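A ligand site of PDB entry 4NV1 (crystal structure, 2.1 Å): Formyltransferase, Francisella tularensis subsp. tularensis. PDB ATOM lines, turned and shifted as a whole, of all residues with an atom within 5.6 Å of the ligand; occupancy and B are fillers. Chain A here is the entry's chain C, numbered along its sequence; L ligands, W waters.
O4 of the ligand sits close to NZ of Lys 77.
A ring nitrogen (NE2) of His 217 lies within hydrogen-bond range of an oxygen (O11) of the ligand, 3.4 Å away.
The side-chain amide nitrogen (ND2) of Asn 12 sits at hydrogen-bond distance from an oxygen (O2) of the ligand, 3.4 Å away.
The side-chain amide nitrogen (NE2) of Gln 107 lies within hydrogen-bond range of an oxygen (O12) of the ligand.
The side-chain hydroxyl of Tyr 151 is in hydrogen-bond range of an oxygen (O1) of the ligand (3.0 Å).
An oxygen (O9) of the ligand is in hydrogen-bond range of the side-chain hydroxyl (OH) of Tyr 220 (3.0 Å).
ND1 of His 75 is in hydrogen-bond range of O1 of the ligand (2.9 Å).
O13 of the ligand is in hydrogen-bond range of ND2 of Asn 222 (2.7 Å).
The side-chain amide nitrogen (NE2) of Gln 107 is in hydrogen-bond range of the side-chain hydroxyl (OG) of Ser 147 (2.8 Å).
The side-chain carboxylate of Asp 11 sits at hydrogen-bond distance from the backbone NH of Lys 77.
NE2 of Gln 155 lies close to OH of Tyr 151, at 3.3 Å.
The backbone carbonyl oxygen of Met 215 lies within hydrogen-bond range of the side-chain amide nitrogen of Asn 222 (3.0 Å).
ND1 of His 217 lies within hydrogen-bond range of OG of Ser 147.
The side-chain amide oxygen (OD1) of Asn 222 sits close to the side-chain hydroxyl (OH) of Tyr 191, at 3.3 Å.
ND1 of His 75 sits close to OH of Tyr 151 (3.4 Å).
N of Asp 11 sits at hydrogen-bond distance from O of His 75 (2.8 Å).
Merely in contact with the ligand: Ser 76, Trp 104, Phe 105 and Tyr 191.
Hydrophobic or aromatic side chains within 4 Å of the ligand: His 75, Trp 104, Phe 105, Tyr 151, His 217 and Tyr 220.
The nearest printed residue that does not touch the ligand is Ser 147 (4.2 Å).
Water W2 bridges O9 of the ligand (2.4 Å) and OH of Tyr 220 (3.2 Å).
Water W1 lies within hydrogen-bond range of ND2 of Asn 222 (3.1 Å), O13 of the ligand (3.2 Å) and O of Met 215 (3.5 Å).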
ATOM      1  N   ASP A  11       8.022 -35.168 -10.256  1.00  0.00           N
ATOM      2  CA  ASP A  11       7.115 -35.041  -9.145  1.00  0.00           C
ATOM      3  C   ASP A  11       5.771 -35.708  -9.391  1.00  0.00           C
ATOM      4  O   ASP A  11       4.802 -35.279  -8.796  1.00  0.00           O
ATOM      5  CB  ASP A  11       6.975 -33.571  -8.840  1.00  0.00           C
ATOM      6  CG  ASP A  11       8.284 -33.012  -8.334  1.00  0.00           C
ATOM      7  OD1 ASP A  11       8.692 -33.501  -7.290  1.00  0.00           O
ATOM      8  OD2 ASP A  11       8.933 -32.176  -8.999  1.00  0.00           O
ATOM      9  N   ASN A  12       5.703 -36.770 -10.179  1.00  0.00           N
ATOM     10  CA  ASN A  12       4.416 -37.425 -10.448  1.00  0.00           C
ATOM     11  C   ASN A  12       4.457 -38.860 -10.095  1.00  0.00           C
ATOM     12  O   ASN A  12       5.318 -39.555 -10.602  1.00  0.00           O
ATOM     13  CB  ASN A  12       4.101 -37.450 -11.950  1.00  0.00           C
ATOM     14  CG  ASN A  12       2.691 -37.952 -12.253  1.00  0.00           C
ATOM     15  OD1 ASN A  12       2.404 -39.151 -12.318  1.00  0.00           O
ATOM     16  ND2 ASN A  12       1.820 -37.009 -12.499  1.00  0.00           N
ATOM     17  N   HIS A  75       7.564 -34.346 -15.746  1.00  0.00           N
ATOM     18  CA  HIS A  75       6.514 -33.824 -14.862  1.00  0.00           C
ATOM     19  C   HIS A  75       7.186 -33.449 -13.525  1.00  0.00           C
ATOM     20  O   HIS A  75       6.939 -34.023 -12.512  1.00  0.00           O
ATOM     21  CB  HIS A  75       5.408 -34.834 -14.639  1.00  0.00           C
ATOM     22  CG  HIS A  75       4.432 -34.902 -15.770  1.00  0.00           C
ATOM     23  ND1 HIS A  75       3.276 -34.156 -15.800  1.00  0.00           N
ATOM     24  CD2 HIS A  75       4.432 -35.649 -16.906  1.00  0.00           C
ATOM     25  CE1 HIS A  75       2.584 -34.459 -16.877  1.00  0.00           C
ATOM     26  NE2 HIS A  75       3.259 -35.378 -17.552  1.00  0.00           N
ATOM     27  N   SER A  76       8.115 -32.519 -13.623  1.00  0.00           N
ATOM     28  CA  SER A  76       9.135 -32.320 -12.642  1.00  0.00           C
ATOM     29  C   SER A  76       8.750 -30.935 -12.284  1.00  0.00           C
ATOM     30  O   SER A  76       8.693 -30.123 -13.222  1.00  0.00           O
ATOM     31  CB  SER A  76      10.521 -32.227 -13.313  1.00  0.00           C
ATOM     32  OG  SER A  76      11.450 -31.435 -12.560  1.00  0.00           O
ATOM     33  N   LYS A  77       8.613 -30.632 -10.989  1.00  0.00           N
ATOM     34  CA  LYS A  77       8.431 -29.224 -10.590  1.00  0.00           C
ATOM     35  C   LYS A  77       9.567 -28.271 -10.976  1.00  0.00           C
ATOM     36  O   LYS A  77       9.376 -27.050 -10.985  1.00  0.00           O
ATOM     37  CB  LYS A  77       8.136 -29.114  -9.086  1.00  0.00           C
ATOM     38  CG  LYS A  77       6.852 -29.783  -8.616  1.00  0.00           C
ATOM     39  CD  LYS A  77       6.781 -29.820  -7.086  1.00  0.00           C
ATOM     40  CE  LYS A  77       5.495 -30.381  -6.499  1.00  0.00           C
ATOM     41  NZ  LYS A  77       4.296 -29.804  -7.161  1.00  0.00           N
ATOM     42  N   PRO A  95       4.121 -33.073 -21.463  1.00  0.00           N
ATOM     43  CA  PRO A  95       2.697 -33.073 -21.767  1.00  0.00           C
ATOM     44  C   PRO A  95       2.211 -31.946 -22.654  1.00  0.00           C
ATOM     45  O   PRO A  95       1.090 -31.493 -22.462  1.00  0.00           O
ATOM     46  CB  PRO A  95       2.017 -32.983 -20.383  1.00  0.00           C
ATOM     47  CG  PRO A  95       2.959 -32.158 -19.608  1.00  0.00           C
ATOM     48  CD  PRO A  95       4.363 -32.394 -20.175  1.00  0.00           C
ATOM     49  N   TRP A 104       2.851 -23.135 -19.376  1.00  0.00           N
ATOM     50  CA  TRP A 104       1.879 -23.682 -18.413  1.00  0.00           C
ATOM     51  C   TRP A 104       0.530 -24.212 -18.953  1.00  0.00           C
ATOM     52  O   TRP A 104      -0.140 -23.542 -19.740  1.00  0.00           O
ATOM     53  CB  TRP A 104       1.663 -22.665 -17.276  1.00  0.00           C
ATOM     54  CG  TRP A 104       2.743 -22.865 -16.264  1.00  0.00           C
ATOM     55  CD1 TRP A 104       4.042 -22.449 -16.356  1.00  0.00           C
ATOM     56  CD2 TRP A 104       2.629 -23.607 -15.060  1.00  0.00           C
ATOM     57  NE1 TRP A 104       4.739 -22.870 -15.255  1.00  0.00           N
ATOM     58  CE2 TRP A 104       3.899 -23.582 -14.438  1.00  0.00           C
ATOM     59  CE3 TRP A 104       1.584 -24.292 -14.427  1.00  0.00           C
ATOM     60  CZ2 TRP A 104       4.138 -24.200 -13.216  1.00  0.00           C
ATOM     61  CZ3 TRP A 104       1.836 -24.914 -13.210  1.00  0.00           C
ATOM     62  CH2 TRP A 104       3.095 -24.870 -12.625  1.00  0.00           C
ATOM     63  N   PHE A 105       0.180 -25.420 -18.513  1.00  0.00           N
ATOM     64  CA  PHE A 105      -1.080 -26.100 -18.742  1.00  0.00           C
ATOM     65  C   PHE A 105      -1.481 -26.039 -20.206  1.00  0.00           C
ATOM     66  O   PHE A 105      -2.529 -25.497 -20.532  1.00  0.00           O
ATOM     67  CB  PHE A 105      -2.160 -25.479 -17.884  1.00  0.00           C
ATOM     68  CG  PHE A 105      -1.899 -25.599 -16.405  1.00  0.00           C
ATOM     69  CD1 PHE A 105      -2.409 -24.657 -15.543  1.00  0.00           C
ATOM     70  CD2 PHE A 105      -1.134 -26.628 -15.856  1.00  0.00           C
ATOM     71  CE1 PHE A 105      -2.151 -24.714 -14.183  1.00  0.00           C
ATOM     72  CE2 PHE A 105      -0.894 -26.709 -14.482  1.00  0.00           C
ATOM     73  CZ  PHE A 105      -1.427 -25.759 -13.642  1.00  0.00           C
ATOM     74  N   PRO A 106      -0.638 -26.613 -21.047  1.00  0.00           N
ATOM     75  CA  PRO A 106      -0.780 -26.695 -22.520  1.00  0.00           C
ATOM     76  C   PRO A 106      -2.132 -27.161 -22.917  1.00  0.00           C
ATOM     77  O   PRO A 106      -2.756 -26.526 -23.772  1.00  0.00           O
ATOM     78  CB  PRO A 106       0.310 -27.666 -22.957  1.00  0.00           C
ATOM     79  CG  PRO A 106       0.825 -28.301 -21.686  1.00  0.00           C
ATOM     80  CD  PRO A 106       0.531 -27.377 -20.555  1.00  0.00           C
ATOM     81  N   GLN A 107      -2.650 -28.217 -22.275  1.00  0.00           N
ATOM     82  CA  GLN A 107      -3.958 -28.712 -22.662  1.00  0.00           C
ATOM     83  C   GLN A 107      -5.104 -27.711 -22.383  1.00  0.00           C
ATOM     84  O   GLN A 107      -6.042 -27.578 -23.180  1.00  0.00           O
ATOM     85  CB  GLN A 107      -4.282 -30.139 -22.159  1.00  0.00           C
ATOM     86  CG  GLN A 107      -4.804 -30.236 -20.728  1.00  0.00           C
ATOM     87  CD  GLN A 107      -3.765 -29.901 -19.744  1.00  0.00           C
ATOM     88  OE1 GLN A 107      -2.586 -29.774 -20.095  1.00  0.00           O
ATOM     89  NE2 GLN A 107      -4.144 -29.846 -18.456  1.00  0.00           N
ATOM     90  N   VAL A 108      -4.999 -26.930 -21.306  1.00  0.00           N
ATOM     91  CA  VAL A 108      -5.996 -25.916 -21.063  1.00  0.00           C
ATOM     92  C   VAL A 108      -6.026 -24.936 -22.214  1.00  0.00           C
ATOM     93  O   VAL A 108      -7.074 -24.698 -22.830  1.00  0.00           O
ATOM     94  CB  VAL A 108      -5.778 -25.178 -19.745  1.00  0.00           C
ATOM     95  CG1 VAL A 108      -6.815 -24.089 -19.605  1.00  0.00           C
ATOM     96  CG2 VAL A 108      -5.834 -26.116 -18.563  1.00  0.00           C
ATOM     97  N   SER A 147     -10.144 -30.488 -19.234  1.00  0.00           N
ATOM     98  CA  SER A 147      -8.711 -30.519 -18.994  1.00  0.00           C
ATOM     99  C   SER A 147      -8.213 -31.826 -18.436  1.00  0.00           C
ATOM    100  O   SER A 147      -7.099 -32.265 -18.776  1.00  0.00           O
ATOM    101  CB  SER A 147      -8.197 -29.342 -18.173  1.00  0.00           C
ATOM    102  OG  SER A 147      -6.847 -29.548 -17.643  1.00  0.00           O
ATOM    103  N   TYR A 151      -5.508 -34.130 -20.358  1.00  0.00           N
ATOM    104  CA  TYR A 151      -4.257 -34.331 -19.678  1.00  0.00           C
ATOM    105  C   TYR A 151      -4.018 -35.824 -19.558  1.00  0.00           C
ATOM    106  O   TYR A 151      -2.858 -36.291 -19.691  1.00  0.00           O
ATOM    107  CB  TYR A 151      -4.314 -33.721 -18.290  1.00  0.00           C
ATOM    108  CG  TYR A 151      -3.129 -33.931 -17.344  1.00  0.00           C
ATOM    109  CD1 TYR A 151      -2.061 -33.027 -17.350  1.00  0.00           C
ATOM    110  CD2 TYR A 151      -3.142 -34.914 -16.372  1.00  0.00           C
ATOM    111  CE1 TYR A 151      -1.008 -33.140 -16.455  1.00  0.00           C
ATOM    112  CE2 TYR A 151      -2.090 -35.028 -15.444  1.00  0.00           C
ATOM    113  CZ  TYR A 151      -1.016 -34.147 -15.511  1.00  0.00           C
ATOM    114  OH  TYR A 151       0.052 -34.190 -14.632  1.00  0.00           O
ATOM    115  N   GLN A 155      -0.821 -37.839 -20.990  1.00  0.00           N
ATOM    116  CA  GLN A 155       0.056 -38.558 -20.088  1.00  0.00           C
ATOM    117  C   GLN A 155       0.305 -39.948 -20.545  1.00  0.00           C
ATOM    118  O   GLN A 155       1.441 -40.386 -20.663  1.00  0.00           O
ATOM    119  CB  GLN A 155      -0.426 -38.482 -18.634  1.00  0.00           C
ATOM    120  CG  GLN A 155       0.636 -38.751 -17.615  1.00  0.00           C
ATOM    121  CD  GLN A 155       0.170 -38.487 -16.181  1.00  0.00           C
ATOM    122  OE1 GLN A 155      -0.236 -39.417 -15.488  1.00  0.00           O
ATOM    123  NE2 GLN A 155       0.217 -37.244 -15.737  1.00  0.00           N
ATOM    124  N   TYR A 191      -2.106 -17.877 -17.380  1.00  0.00           N
ATOM    125  CA  TYR A 191      -3.106 -18.766 -16.864  1.00  0.00           C
ATOM    126  C   TYR A 191      -3.964 -17.999 -15.834  1.00  0.00           C
ATOM    127  O   TYR A 191      -5.203 -17.892 -15.966  1.00  0.00           O
ATOM    128  CB  TYR A 191      -2.446 -20.031 -16.245  1.00  0.00           C
ATOM    129  CG  TYR A 191      -3.439 -20.977 -15.622  1.00  0.00           C
ATOM    130  CD1 TYR A 191      -4.280 -21.745 -16.428  1.00  0.00           C
ATOM    131  CD2 TYR A 191      -3.580 -21.092 -14.228  1.00  0.00           C
ATOM    132  CE1 TYR A 191      -5.235 -22.568 -15.877  1.00  0.00           C
ATOM    133  CE2 TYR A 191      -4.528 -21.917 -13.658  1.00  0.00           C
ATOM    134  CZ  TYR A 191      -5.355 -22.659 -14.488  1.00  0.00           C
ATOM    135  OH  TYR A 191      -6.306 -23.512 -13.976  1.00  0.00           O
ATOM    136  N   MET A 215     -11.095 -25.212 -18.083  1.00  0.00           N
ATOM    137  CA  MET A 215     -10.823 -24.902 -16.692  1.00  0.00           C
ATOM    138  C   MET A 215     -11.289 -25.906 -15.637  1.00  0.00           C
ATOM    139  O   MET A 215     -11.101 -25.660 -14.440  1.00  0.00           O
ATOM    140  CB  MET A 215     -11.432 -23.534 -16.354  1.00  0.00           C
ATOM    141  CG  MET A 215     -10.912 -22.349 -17.129  1.00  0.00           C
ATOM    142  SD  MET A 215      -9.169 -21.957 -16.958  1.00  0.00           S
ATOM    143  CE  MET A 215      -9.142 -21.051 -15.447  1.00  0.00           C
ATOM    144  N   HIS A 217     -10.825 -29.521 -14.051  1.00  0.00           N
ATOM    145  CA  HIS A 217      -9.795 -30.508 -13.800  1.00  0.00           C
ATOM    146  C   HIS A 217      -9.884 -30.880 -12.295  1.00  0.00           C
ATOM    147  O   HIS A 217      -9.143 -30.280 -11.507  1.00  0.00           O
ATOM    148  CB  HIS A 217      -8.439 -29.917 -14.149  1.00  0.00           C
ATOM    149  CG  HIS A 217      -7.362 -30.943 -14.349  1.00  0.00           C
ATOM    150  ND1 HIS A 217      -6.620 -31.037 -15.508  1.00  0.00           N
ATOM    151  CD2 HIS A 217      -6.912 -31.945 -13.537  1.00  0.00           C
ATOM    152  CE1 HIS A 217      -5.778 -32.055 -15.415  1.00  0.00           C
ATOM    153  NE2 HIS A 217      -5.941 -32.617 -14.227  1.00  0.00           N
ATOM    154  N   TYR A 220      -9.066 -29.784  -8.761  1.00  0.00           N
ATOM    155  CA  TYR A 220      -8.734 -28.388  -8.573  1.00  0.00           C
ATOM    156  C   TYR A 220      -9.939 -27.430  -8.713  1.00  0.00           C
ATOM    157  O   TYR A 220     -10.909 -27.705  -9.410  1.00  0.00           O
ATOM    158  CB  TYR A 220      -7.610 -27.987  -9.513  1.00  0.00           C
ATOM    159  CG  TYR A 220      -6.363 -28.819  -9.315  1.00  0.00           C
ATOM    160  CD1 TYR A 220      -6.080 -29.859 -10.166  1.00  0.00           C
ATOM    161  CD2 TYR A 220      -5.514 -28.605  -8.240  1.00  0.00           C
ATOM    162  CE1 TYR A 220      -4.931 -30.598 -10.033  1.00  0.00           C
ATOM    163  CE2 TYR A 220      -4.357 -29.347  -8.089  1.00  0.00           C
ATOM    164  CZ  TYR A 220      -4.080 -30.346  -8.997  1.00  0.00           C
ATOM    165  OH  TYR A 220      -2.959 -31.142  -8.905  1.00  0.00           O
ATOM    166  N   LYS A 221      -9.803 -26.280  -8.081  1.00  0.00           N
ATOM    167  CA  LYS A 221     -10.725 -25.170  -8.181  1.00  0.00           C
ATOM    168  C   LYS A 221     -10.030 -24.099  -8.991  1.00  0.00           C
ATOM    169  O   LYS A 221      -9.085 -23.565  -8.472  1.00  0.00           O
ATOM    170  CB  LYS A 221     -11.032 -24.599  -6.785  1.00  0.00           C
ATOM    171  CG  LYS A 221     -11.685 -25.626  -5.876  1.00  0.00           C
ATOM    172  CD  LYS A 221     -12.777 -25.002  -5.013  1.00  0.00           C
ATOM    173  CE  LYS A 221     -13.247 -25.989  -3.943  1.00  0.00           C
ATOM    174  NZ  LYS A 221     -13.411 -27.362  -4.501  1.00  0.00           N
ATOM    175  N   ASN A 222     -10.537 -23.774 -10.195  1.00  0.00           N
ATOM    176  CA  ASN A 222      -9.893 -22.869 -11.131  1.00  0.00           C
ATOM    177  C   ASN A 222     -10.639 -21.613 -11.509  1.00  0.00           C
ATOM    178  O   ASN A 222     -10.226 -20.517 -11.118  1.00  0.00           O
ATOM    179  CB  ASN A 222      -9.464 -23.631 -12.412  1.00  0.00           C
ATOM    180  CG  ASN A 222      -8.496 -24.755 -12.114  1.00  0.00           C
ATOM    181  OD1 ASN A 222      -7.651 -24.632 -11.183  1.00  0.00           O
ATOM    182  ND2 ASN A 222      -8.625 -25.883 -12.800  1.00  0.00           N
HETATM  183  O1  LIG L   1       1.990 -31.909 -14.411  1.00  0.00           O
HETATM  184  P1  LIG L   1       2.220 -32.287 -12.928  1.00  0.00           P
HETATM  185  O2  LIG L   1       2.036 -33.651 -12.286  1.00  0.00           O
HETATM  186  O3  LIG L   1       3.168 -31.239 -12.185  1.00  0.00           O
HETATM  187  C1  LIG L   1       4.537 -31.152 -12.500  1.00  0.00           C
HETATM  188  C2  LIG L   1       4.922 -29.971 -11.626  1.00  0.00           C
HETATM  189  O4  LIG L   1       4.312 -30.050 -10.331  1.00  0.00           O
HETATM  190  C3  LIG L   1       4.530 -28.659 -12.259  1.00  0.00           C
HETATM  191  O5  LIG L   1       5.152 -27.689 -11.396  1.00  0.00           O
HETATM  192  C4  LIG L   1       5.018 -28.647 -13.723  1.00  0.00           C
HETATM  193  N1  LIG L   1       4.773 -27.381 -14.391  1.00  0.00           N
HETATM  194  C5  LIG L   1       4.432 -29.786 -14.552  1.00  0.00           C
HETATM  195  C6  LIG L   1       4.976 -29.786 -15.975  1.00  0.00           C
HETATM  196  O6  LIG L   1       4.793 -31.015 -13.904  1.00  0.00           O
HETATM  197  O7  LIG L   1       1.087 -31.915 -11.860  1.00  0.00           O
HETATM  198  P2  LIG L   1       0.176 -30.655 -11.580  1.00  0.00           P
HETATM  199  O8  LIG L   1       0.851 -29.473 -10.922  1.00  0.00           O
HETATM  200  O9  LIG L   1      -0.925 -31.551 -11.013  1.00  0.00           O
HETATM  201  O10 LIG L   1      -0.560 -30.185 -12.940  1.00  0.00           O
HETATM  202  C7  LIG L   1      -1.307 -31.171 -13.657  1.00  0.00           C
HETATM  203  C8  LIG L   1      -2.568 -30.589 -14.283  1.00  0.00           C
HETATM  204  O11 LIG L   1      -3.518 -30.357 -13.268  1.00  0.00           O
HETATM  205  C9  LIG L   1      -2.407 -29.276 -14.977  1.00  0.00           C
HETATM  206  O12 LIG L   1      -2.161 -29.418 -16.389  1.00  0.00           O
HETATM  207  C10 LIG L   1      -3.808 -28.655 -14.874  1.00  0.00           C
HETATM  208  C11 LIG L   1      -4.311 -29.216 -13.547  1.00  0.00           C
HETATM  209  N2  LIG L   1      -4.281 -28.170 -12.528  1.00  0.00           N
HETATM  210  C12 LIG L   1      -3.185 -28.027 -11.751  1.00  0.00           C
HETATM  211  C13 LIG L   1      -3.141 -27.021 -10.798  1.00  0.00           C
HETATM  212  C14 LIG L   1      -1.953 -26.725  -9.903  1.00  0.00           C
HETATM  213  C15 LIG L   1      -5.349 -27.369 -12.367  1.00  0.00           C
HETATM  214  O13 LIG L   1      -6.478 -27.511 -13.098  1.00  0.00           O
HETATM  215  N3  LIG L   1      -5.399 -26.415 -11.428  1.00  0.00           N
HETATM  216  C16 LIG L   1      -4.283 -26.277 -10.671  1.00  0.00           C
HETATM  217  O14 LIG L   1      -4.202 -25.327  -9.743  1.00  0.00           O
HETATM  218  O   HOH W   1      -8.058 -26.730 -15.734  1.00  0.00           O
HETATM  219  O   HOH W   2      -2.467 -33.422 -11.089  1.00  0.00           O
